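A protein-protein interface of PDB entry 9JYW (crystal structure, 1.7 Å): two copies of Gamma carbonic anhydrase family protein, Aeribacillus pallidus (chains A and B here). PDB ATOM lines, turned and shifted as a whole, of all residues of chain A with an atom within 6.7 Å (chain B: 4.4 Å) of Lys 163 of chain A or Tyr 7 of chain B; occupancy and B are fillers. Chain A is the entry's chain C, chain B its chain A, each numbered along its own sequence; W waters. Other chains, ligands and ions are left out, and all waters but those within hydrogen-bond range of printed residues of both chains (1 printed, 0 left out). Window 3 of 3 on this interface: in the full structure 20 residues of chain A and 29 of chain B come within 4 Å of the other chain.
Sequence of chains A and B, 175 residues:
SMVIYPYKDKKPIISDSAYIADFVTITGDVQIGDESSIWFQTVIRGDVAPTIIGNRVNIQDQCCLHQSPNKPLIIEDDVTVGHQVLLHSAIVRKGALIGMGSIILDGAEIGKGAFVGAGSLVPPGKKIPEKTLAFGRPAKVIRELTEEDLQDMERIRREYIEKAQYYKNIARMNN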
ATOM      1  N   TYR A  19      20.943  31.375 -11.180  1.00  0.00           N
ATOM      2  CA  TYR A  19      20.340  32.272 -12.183  1.00  0.00           C
ATOM      3  C   TYR A  19      19.453  33.267 -11.450  1.00  0.00           C
ATOM      4  O   TYR A  19      18.588  32.796 -10.709  1.00  0.00           O
ATOM      5  CB  TYR A  19      19.536  31.484 -13.208  1.00  0.00           C
ATOM      6  CG  TYR A  19      18.664  32.321 -14.119  1.00  0.00           C
ATOM      7  CD1 TYR A  19      19.190  33.409 -14.807  1.00  0.00           C
ATOM      8  CD2 TYR A  19      17.319  32.055 -14.264  1.00  0.00           C
ATOM      9  CE1 TYR A  19      18.404  34.174 -15.653  1.00  0.00           C
ATOM     10  CE2 TYR A  19      16.514  32.804 -15.109  1.00  0.00           C
ATOM     11  CZ  TYR A  19      17.060  33.859 -15.805  1.00  0.00           C
ATOM     12  OH  TYR A  19      16.266  34.630 -16.624  1.00  0.00           O
ATOM     13  N   TRP A  39      13.285  33.530 -10.440  1.00  0.00           N
ATOM     14  CA  TRP A  39      12.655  33.868 -11.739  1.00  0.00           C
ATOM     15  C   TRP A  39      12.059  35.281 -11.707  1.00  0.00           C
ATOM     16  O   TRP A  39      12.038  35.943 -10.670  1.00  0.00           O
ATOM     17  CB  TRP A  39      11.670  32.756 -12.143  1.00  0.00           C
ATOM     18  CG  TRP A  39      12.410  31.515 -12.513  1.00  0.00           C
ATOM     19  CD1 TRP A  39      12.934  30.576 -11.664  1.00  0.00           C
ATOM     20  CD2 TRP A  39      12.848  31.159 -13.830  1.00  0.00           C
ATOM     21  NE1 TRP A  39      13.629  29.638 -12.369  1.00  0.00           N
ATOM     22  CE2 TRP A  39      13.596  29.961 -13.705  1.00  0.00           C
ATOM     23  CE3 TRP A  39      12.655  31.723 -15.090  1.00  0.00           C
ATOM     24  CZ2 TRP A  39      14.156  29.331 -14.812  1.00  0.00           C
ATOM     25  CZ3 TRP A  39      13.206  31.087 -16.179  1.00  0.00           C
ATOM     26  CH2 TRP A  39      13.959  29.913 -16.041  1.00  0.00           C
ATOM     27  N   ARG A 158      14.178  19.289 -12.437  1.00  0.00           N
ATOM     28  CA  ARG A 158      15.299  19.103 -13.396  1.00  0.00           C
ATOM     29  C   ARG A 158      15.105  20.057 -14.587  1.00  0.00           C
ATOM     30  O   ARG A 158      16.116  20.700 -15.031  1.00  0.00           O
ATOM     31  CB  ARG A 158      15.390  17.651 -13.866  1.00  0.00           C
ATOM     32  CG  ARG A 158      16.371  17.494 -15.026  1.00  0.00           C
ATOM     33  CD  ARG A 158      16.388  16.186 -15.791  1.00  0.00           C
ATOM     34  NE  ARG A 158      15.139  15.889 -16.492  1.00  0.00           N
ATOM     35  CZ  ARG A 158      14.157  15.127 -16.011  1.00  0.00           C
ATOM     36  NH1 ARG A 158      14.260  14.587 -14.807  1.00  0.00           N
ATOM     37  NH2 ARG A 158      13.049  14.952 -16.710  1.00  0.00           N
ATOM     38  N   GLU A 159      13.856  20.185 -15.054  1.00  0.00           N
ATOM     39  CA  GLU A 159      13.541  21.082 -16.196  1.00  0.00           C
ATOM     40  C   GLU A 159      13.918  22.523 -15.828  1.00  0.00           C
ATOM     41  O   GLU A 159      14.480  23.236 -16.689  1.00  0.00           O
ATOM     42  CB  GLU A 159      12.082  20.926 -16.623  1.00  0.00           C
ATOM     43  CG  GLU A 159      11.842  19.638 -17.432  1.00  0.00           C
ATOM     44  CD  GLU A 159      12.931  19.297 -18.453  1.00  0.00           C
ATOM     45  OE1 GLU A 159      13.329  20.220 -19.201  1.00  0.00           O
ATOM     46  OE2 GLU A 159      13.420  18.124 -18.479  1.00  0.00           O
ATOM     47  N   TYR A 160      13.673  22.943 -14.585  1.00  0.00           N
ATOM     48  CA  TYR A 160      13.994  24.338 -14.171  1.00  0.00           C
ATOM     49  C   TYR A 160      15.515  24.576 -14.147  1.00  0.00           C
ATOM     50  O   TYR A 160      15.990  25.655 -14.532  1.00  0.00           O
ATOM     51  CB  TYR A 160      13.301  24.677 -12.854  1.00  0.00           C
ATOM     52  CG  TYR A 160      12.000  25.396 -13.089  1.00  0.00           C
ATOM     53  CD1 TYR A 160      11.998  26.754 -13.363  1.00  0.00           C
ATOM     54  CD2 TYR A 160      10.801  24.718 -13.098  1.00  0.00           C
ATOM     55  CE1 TYR A 160      10.820  27.440 -13.628  1.00  0.00           C
ATOM     56  CE2 TYR A 160       9.608  25.381 -13.356  1.00  0.00           C
ATOM     57  CZ  TYR A 160       9.619  26.743 -13.607  1.00  0.00           C
ATOM     58  OH  TYR A 160       8.467  27.408 -13.893  1.00  0.00           O
ATOM     59  N   ILE A 161      16.296  23.596 -13.729  1.00  0.00           N
ATOM     60  CA  ILE A 161      17.741  23.769 -13.750  1.00  0.00           C
ATOM     61  C   ILE A 161      18.264  24.062 -15.131  1.00  0.00           C
ATOM     62  O   ILE A 161      19.103  24.904 -15.319  1.00  0.00           O
ATOM     63  CB  ILE A 161      18.462  22.520 -13.180  1.00  0.00           C
ATOM     64  CG1 ILE A 161      18.101  22.343 -11.709  1.00  0.00           C
ATOM     65  CG2 ILE A 161      19.962  22.637 -13.356  1.00  0.00           C
ATOM     66  CD1 ILE A 161      18.673  21.094 -11.087  1.00  0.00           C
ATOM     67  N   GLU A 162      17.749  23.321 -16.094  1.00  0.00           N
ATOM     68  CA  GLU A 162      18.205  23.486 -17.448  1.00  0.00           C
ATOM     69  C   GLU A 162      17.732  24.784 -18.075  1.00  0.00           C
ATOM     70  O   GLU A 162      18.476  25.446 -18.747  1.00  0.00           O
ATOM     71  CB  GLU A 162      17.722  22.335 -18.296  1.00  0.00           C
ATOM     72  CG  GLU A 162      18.410  21.026 -17.951  1.00  0.00           C
ATOM     73  CD  GLU A 162      17.736  19.840 -18.598  1.00  0.00           C
ATOM     74  OE1 GLU A 162      16.549  19.974 -18.925  1.00  0.00           O
ATOM     75  OE2 GLU A 162      18.377  18.782 -18.769  1.00  0.00           O
ATOM     76  N   LYS A 163      16.463  25.109 -17.861  1.00  0.00           N
ATOM     77  CA  LYS A 163      15.973  26.401 -18.396  1.00  0.00           C
ATOM     78  C   LYS A 163      16.725  27.567 -17.791  1.00  0.00           C
ATOM     79  O   LYS A 163      17.005  28.531 -18.458  1.00  0.00           O
ATOM     80  CB  LYS A 163      14.477  26.561 -18.208  1.00  0.00           C
ATOM     81  CG  LYS A 163      13.639  25.494 -18.880  1.00  0.00           C
ATOM     82  CD  LYS A 163      12.323  26.071 -19.359  1.00  0.00           C
ATOM     83  CE  LYS A 163      11.310  24.976 -19.642  1.00  0.00           C
ATOM     84  NZ  LYS A 163      11.612  24.214 -20.873  1.00  0.00           N
ATOM     85  N   ALA A 164      17.012  27.473 -16.494  1.00  0.00           N
ATOM     86  CA  ALA A 164      17.809  28.517 -15.810  1.00  0.00           C
ATOM     87  C   ALA A 164      19.149  28.693 -16.550  1.00  0.00           C
ATOM     88  O   ALA A 164      19.573  29.842 -16.779  1.00  0.00           O
ATOM     89  CB  ALA A 164      18.009  28.187 -14.362  1.00  0.00           C
ATOM     90  N   GLN A 165      19.802  27.590 -16.912  1.00  0.00           N
ATOM     91  CA  GLN A 165      21.119  27.647 -17.607  1.00  0.00           C
ATOM     92  C   GLN A 165      20.919  28.356 -18.962  1.00  0.00           C
ATOM     93  O   GLN A 165      21.757  29.220 -19.307  1.00  0.00           O
ATOM     94  CB  GLN A 165      21.723  26.247 -17.727  1.00  0.00           C
ATOM     95  CG  GLN A 165      22.147  25.613 -16.415  1.00  0.00           C
ATOM     96  CD  GLN A 165      22.705  24.228 -16.656  1.00  0.00           C
ATOM     97  OE1 GLN A 165      23.138  23.902 -17.765  1.00  0.00           O
ATOM     98  NE2 GLN A 165      22.709  23.400 -15.620  1.00  0.00           N
ATOM     99  N   TYR A 166      19.816  28.077 -19.655  1.00  0.00           N
ATOM    100  CA  TYR A 166      19.505  28.654 -20.982  1.00  0.00           C
ATOM    101  C   TYR A 166      19.360  30.180 -20.842  1.00  0.00           C
ATOM    102  O   TYR A 166      20.048  30.964 -21.558  1.00  0.00           O
ATOM    103  CB  TYR A 166      18.291  28.008 -21.653  1.00  0.00           C
ATOM    104  CG  TYR A 166      17.928  28.759 -22.918  1.00  0.00           C
ATOM    105  CD1 TYR A 166      18.500  28.453 -24.146  1.00  0.00           C
ATOM    106  CD2 TYR A 166      17.108  29.876 -22.853  1.00  0.00           C
ATOM    107  CE1 TYR A 166      18.195  29.181 -25.286  1.00  0.00           C
ATOM    108  CE2 TYR A 166      16.820  30.635 -23.973  1.00  0.00           C
ATOM    109  CZ  TYR A 166      17.363  30.289 -25.195  1.00  0.00           C
ATOM    110  OH  TYR A 166      17.062  31.076 -26.282  1.00  0.00           O
ATOM    111  N   TYR A 167      18.488  30.645 -19.931  1.00  0.00           N
ATOM    112  CA  TYR A 167      18.239  32.091 -19.808  1.00  0.00           C
ATOM    113  C   TYR A 167      19.480  32.838 -19.293  1.00  0.00           C
ATOM    114  O   TYR A 167      19.754  33.990 -19.732  1.00  0.00           O
ATOM    115  CB  TYR A 167      17.029  32.338 -18.926  1.00  0.00           C
ATOM    116  CG  TYR A 167      15.704  32.097 -19.596  1.00  0.00           C
ATOM    117  CD1 TYR A 167      15.176  32.980 -20.531  1.00  0.00           C
ATOM    118  CD2 TYR A 167      14.953  30.997 -19.252  1.00  0.00           C
ATOM    119  CE1 TYR A 167      13.965  32.708 -21.159  1.00  0.00           C
ATOM    120  CE2 TYR A 167      13.714  30.752 -19.826  1.00  0.00           C
ATOM    121  CZ  TYR A 167      13.180  31.656 -20.719  1.00  0.00           C
ATOM    122  OH  TYR A 167      11.947  31.367 -21.239  1.00  0.00           O
ATOM    123  N   LYS A 168      20.220  32.229 -18.363  1.00  0.00           N
ATOM    124  CA  LYS A 168      21.446  32.859 -17.821  1.00  0.00           C
ATOM    125  C   LYS A 168      22.402  33.161 -18.987  1.00  0.00           C
ATOM    126  O   LYS A 168      23.014  34.242 -18.985  1.00  0.00           O
ATOM    127  CB  LYS A 168      22.122  31.978 -16.774  1.00  0.00           C
ATOM    128  CG  LYS A 168      23.264  32.675 -16.048  1.00  0.00           C
ATOM    129  CD  LYS A 168      23.768  31.835 -14.897  1.00  0.00           C
ATOM    130  CE  LYS A 168      24.906  32.480 -14.136  1.00  0.00           C
ATOM    131  NZ  LYS A 168      24.389  33.612 -13.355  1.00  0.00           N
ATOM    132  N   ILE A 170      21.437  33.514 -22.347  1.00  0.00           N
ATOM    133  CA  ILE A 170      20.731  34.518 -23.207  1.00  0.00           C
ATOM    134  C   ILE A 170      20.894  35.919 -22.595  1.00  0.00           C
ATOM    135  O   ILE A 170      21.195  36.871 -23.358  1.00  0.00           O
ATOM    136  CB  ILE A 170      19.243  34.147 -23.383  1.00  0.00           C
ATOM    137  CG1 ILE A 170      19.071  32.949 -24.309  1.00  0.00           C
ATOM    138  CG2 ILE A 170      18.416  35.335 -23.859  1.00  0.00           C
ATOM    139  CD1 ILE A 170      19.826  33.042 -25.625  1.00  0.00           C
ATOM    140  N   TYR B   5      12.735  37.940 -24.901  1.00  0.00           N
ATOM    141  CA  TYR B   5      13.773  36.984 -25.228  1.00  0.00           C
ATOM    142  C   TYR B   5      13.303  35.831 -26.069  1.00  0.00           C
ATOM    143  O   TYR B   5      12.152  35.478 -26.001  1.00  0.00           O
ATOM    144  CB  TYR B   5      14.296  36.295 -23.954  1.00  0.00           C
ATOM    145  CG  TYR B   5      15.077  37.124 -22.957  1.00  0.00           C
ATOM    146  CD1 TYR B   5      15.964  38.095 -23.368  1.00  0.00           C
ATOM    147  CD2 TYR B   5      14.957  36.890 -21.599  1.00  0.00           C
ATOM    148  CE1 TYR B   5      16.689  38.837 -22.452  1.00  0.00           C
ATOM    149  CE2 TYR B   5      15.675  37.623 -20.678  1.00  0.00           C
ATOM    150  CZ  TYR B   5      16.544  38.593 -21.107  1.00  0.00           C
ATOM    151  OH  TYR B   5      17.271  39.317 -20.194  1.00  0.00           O
ATOM    152  N   PRO B   6      14.192  35.280 -26.898  1.00  0.00           N
ATOM    153  CA  PRO B   6      13.880  34.038 -27.587  1.00  0.00           C
ATOM    154  C   PRO B   6      13.958  32.876 -26.594  1.00  0.00           C
ATOM    155  O   PRO B   6      14.553  33.017 -25.517  1.00  0.00           O
ATOM    156  CB  PRO B   6      15.005  33.906 -28.635  1.00  0.00           C
ATOM    157  CG  PRO B   6      16.176  34.583 -27.957  1.00  0.00           C
ATOM    158  CD  PRO B   6      15.581  35.736 -27.169  1.00  0.00           C
ATOM    159  N   TYR B   7      13.345  31.758 -26.947  1.00  0.00           N
ATOM    160  CA  TYR B   7      13.600  30.466 -26.277  1.00  0.00           C
ATOM    161  C   TYR B   7      13.879  29.417 -27.360  1.00  0.00           C
ATOM    162  O   TYR B   7      12.953  29.041 -28.084  1.00  0.00           O
ATOM    163  CB  TYR B   7      12.477  30.054 -25.325  1.00  0.00           C
ATOM    164  CG  TYR B   7      12.839  28.791 -24.577  1.00  0.00           C
ATOM    165  CD1 TYR B   7      13.754  28.805 -23.544  1.00  0.00           C
ATOM    166  CD2 TYR B   7      12.286  27.580 -24.939  1.00  0.00           C
ATOM    167  CE1 TYR B   7      14.121  27.635 -22.902  1.00  0.00           C
ATOM    168  CE2 TYR B   7      12.622  26.407 -24.291  1.00  0.00           C
ATOM    169  CZ  TYR B   7      13.546  26.434 -23.271  1.00  0.00           C
ATOM    170  OH  TYR B   7      13.861  25.254 -22.654  1.00  0.00           O
ATOM    171  N   LYS B   8      15.137  29.004 -27.478  1.00  0.00           N
ATOM    172  CA  LYS B   8      15.619  28.061 -28.519  1.00  0.00           C
ATOM    173  C   LYS B   8      15.208  28.617 -29.889  1.00  0.00           C
ATOM    174  O   LYS B   8      15.595  29.758 -30.183  1.00  0.00           O
ATOM    175  CB  LYS B   8      15.081  26.671 -28.186  1.00  0.00           C
ATOM    176  CG  LYS B   8      15.493  26.120 -26.835  1.00  0.00           C
ATOM    177  CD  LYS B   8      15.361  24.621 -26.787  1.00  0.00           C
ATOM    178  CE  LYS B   8      16.150  23.959 -25.682  1.00  0.00           C
ATOM    179  NZ  LYS B   8      15.395  22.810 -25.129  1.00  0.00           N
ATOM    180  N   ASP B   9      14.405  27.887 -30.657  1.00  0.00           N
ATOM    181  CA  ASP B   9      14.049  28.249 -32.054  1.00  0.00           C
ATOM    182  C   ASP B   9      12.818  29.171 -32.109  1.00  0.00           C
ATOM    183  O   ASP B   9      12.362  29.452 -33.222  1.00  0.00           O
ATOM    184  CB  ASP B   9      13.774  26.987 -32.875  1.00  0.00           C
ATOM    185  CG  ASP B   9      12.680  26.105 -32.280  1.00  0.00           C
ATOM    186  OD1 ASP B   9      12.733  25.846 -31.054  1.00  0.00           O
ATOM    187  OD2 ASP B   9      11.771  25.688 -33.042  1.00  0.00           O
ATOM    188  N   LYS B  10      12.287  29.624 -30.969  1.00  0.00           N
ATOM    189  CA  LYS B  10      11.007  30.375 -30.911  1.00  0.00           C
ATOM    190  C   LYS B  10      11.288  31.781 -30.403  1.00  0.00           C
ATOM    191  O   LYS B  10      12.025  31.925 -29.400  1.00  0.00           O
ATOM    192  CB  LYS B  10       9.998  29.637 -30.026  1.00  0.00           C
ATOM    193  CG  LYS B  10       9.510  28.294 -30.576  1.00  0.00           C
ATOM    194  CD  LYS B  10       8.696  28.404 -31.848  1.00  0.00           C
ATOM    195  CE  LYS B  10       8.214  27.063 -32.366  1.00  0.00           C
ATOM    196  NZ  LYS B  10       7.044  27.216 -33.268  1.00  0.00           N
ATOM    197  N   GLY B  28      10.083  33.426 -25.737  1.00  0.00           N
ATOM    198  CA  GLY B  28       9.832  32.160 -26.434  1.00  0.00           C
ATOM    199  C   GLY B  28       8.601  32.210 -27.317  1.00  0.00           C
ATOM    200  O   GLY B  28       8.410  33.208 -28.056  1.00  0.00           O
ATOM    201  N   ASP B  47       8.069  28.948 -22.800  1.00  0.00           N
ATOM    202  CA  ASP B  47       9.233  28.027 -22.854  1.00  0.00           C
ATOM    203  C   ASP B  47       8.842  26.575 -22.561  1.00  0.00           C
ATOM    204  O   ASP B  47       9.766  25.732 -22.457  1.00  0.00           O
ATOM    205  CB  ASP B  47      10.355  28.503 -21.931  1.00  0.00           C
ATOM    206  CG  ASP B  47       9.923  28.812 -20.494  1.00  0.00           C
ATOM    207  OD1 ASP B  47       8.933  28.202 -20.018  1.00  0.00           O
ATOM    208  OD2 ASP B  47      10.617  29.646 -19.863  1.00  0.00           O
ATOM    209  N   VAL B  48       7.545  26.258 -22.419  1.00  0.00           N
ATOM    210  CA  VAL B  48       7.090  24.871 -22.153  1.00  0.00           C
ATOM    211  C   VAL B  48       6.138  24.431 -23.279  1.00  0.00           C
ATOM    212  O   VAL B  48       6.290  23.295 -23.772  1.00  0.00           O
ATOM    213  CB  VAL B  48       6.478  24.717 -20.741  1.00  0.00           C
ATOM    214  CG1 VAL B  48       5.861  23.345 -20.556  1.00  0.00           C
ATOM    215  CG2 VAL B  48       7.509  24.998 -19.693  1.00  0.00           C
HETATM  216  O   HOH W   1      18.178  30.632 -28.382  1.00  0.00           O
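OH of Tyr 167 of chain A sits at hydrogen-bond distance from OD2 of Asp 47 of chain B.
The side-chain hydroxyl (OH) of Tyr 166 of chain A is in hydrogen-bond range of the backbone NH (N) of Lys 8 of chain B (3.1 Å).
The backbone carbonyl oxygen (O) of Pro 6 of chain B lies within hydrogen-bond range of the side-chain hydroxyl (OH) of Tyr 166 of chain A, 3.3 Å away.
The side-chain hydroxyl of Tyr 7 of chain B lies within hydrogen-bond range of the side-chain amino group of Lys 163 of chain A, 3.1 Å away.
The side-chain amino group (NZ) of Lys 163 of chain A lies within hydrogen-bond range of the backbone carbonyl oxygen (O) of Asp 47 of chain B (2.9 Å).
The backbone NH of Gly 28 of chain B lies within hydrogen-bond range of the backbone carbonyl oxygen of Tyr 5 of chain B (2.9 Å).
Val 48 of chain B touches Lys 163 of chain A (CG2 to CE, 3.8 Å).
Tyr 7 of chain B touches Tyr 166 of chain A (CA to OH, 3.5 Å).
OH of Tyr 167 of chain A touches CD1 of Tyr 7 of chain B, at 3.9 Å.
Tyr 5 of chain B touches Ile 170 of chain A.
Lys 163 of chain A touches just these residues of chain B: Tyr 7, Asp 47 and Val 48.
Printed residues of chain A within 4 Å of Tyr 7 of chain B: Lys 163 (3.1 Å), Tyr 166 (3.5 Å) and Tyr 167 (3.9 Å).
Of the printed residues of chain A, Lys 8 of chain B touches Tyr 166.
Printed residues of chain B within 4 Å of Ile 170 of chain A: Tyr 5.
Printed residues of chain A within 4 Å of Tyr 5 of chain B: Ile 170 (3.7 Å).
Gly 28 of chain B touches none of the printed residues of chain A.
Ala 164 of chain A touches none of the printed residues of chain B.
The nearest printed residue of chain B that does not touch Lys 163 of chain A is Lys 8 of chain B (5.9 Å).
Hydrophobic or aromatic side chains of chain B within 4 Å of the printed part of chain A: Tyr 5, Pro 6, Tyr 7 and Val 48.
Of the 14 printed residues of chain A, 4 touch a printed residue of chain B.
Hydrophobic or aromatic side chains of chain A within 4 Å of the printed part of chain B: Tyr 166, Tyr 167 and Ile 170.
Among the printed residues, 9 pairs touch across the chains.
Among the printed residues, no Asp or Glu carboxylate lies within 4 Å of a Lys or Arg side-chain nitrogen of the other chain.
No position is printed for both chains.
Of the 9 pairs that touch across the chains among the printed residues, none has its exchanged pair printed and touching as well.
Water W1 bridges OH of Tyr 166 of chain A and O of Lys 8 of chain B.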
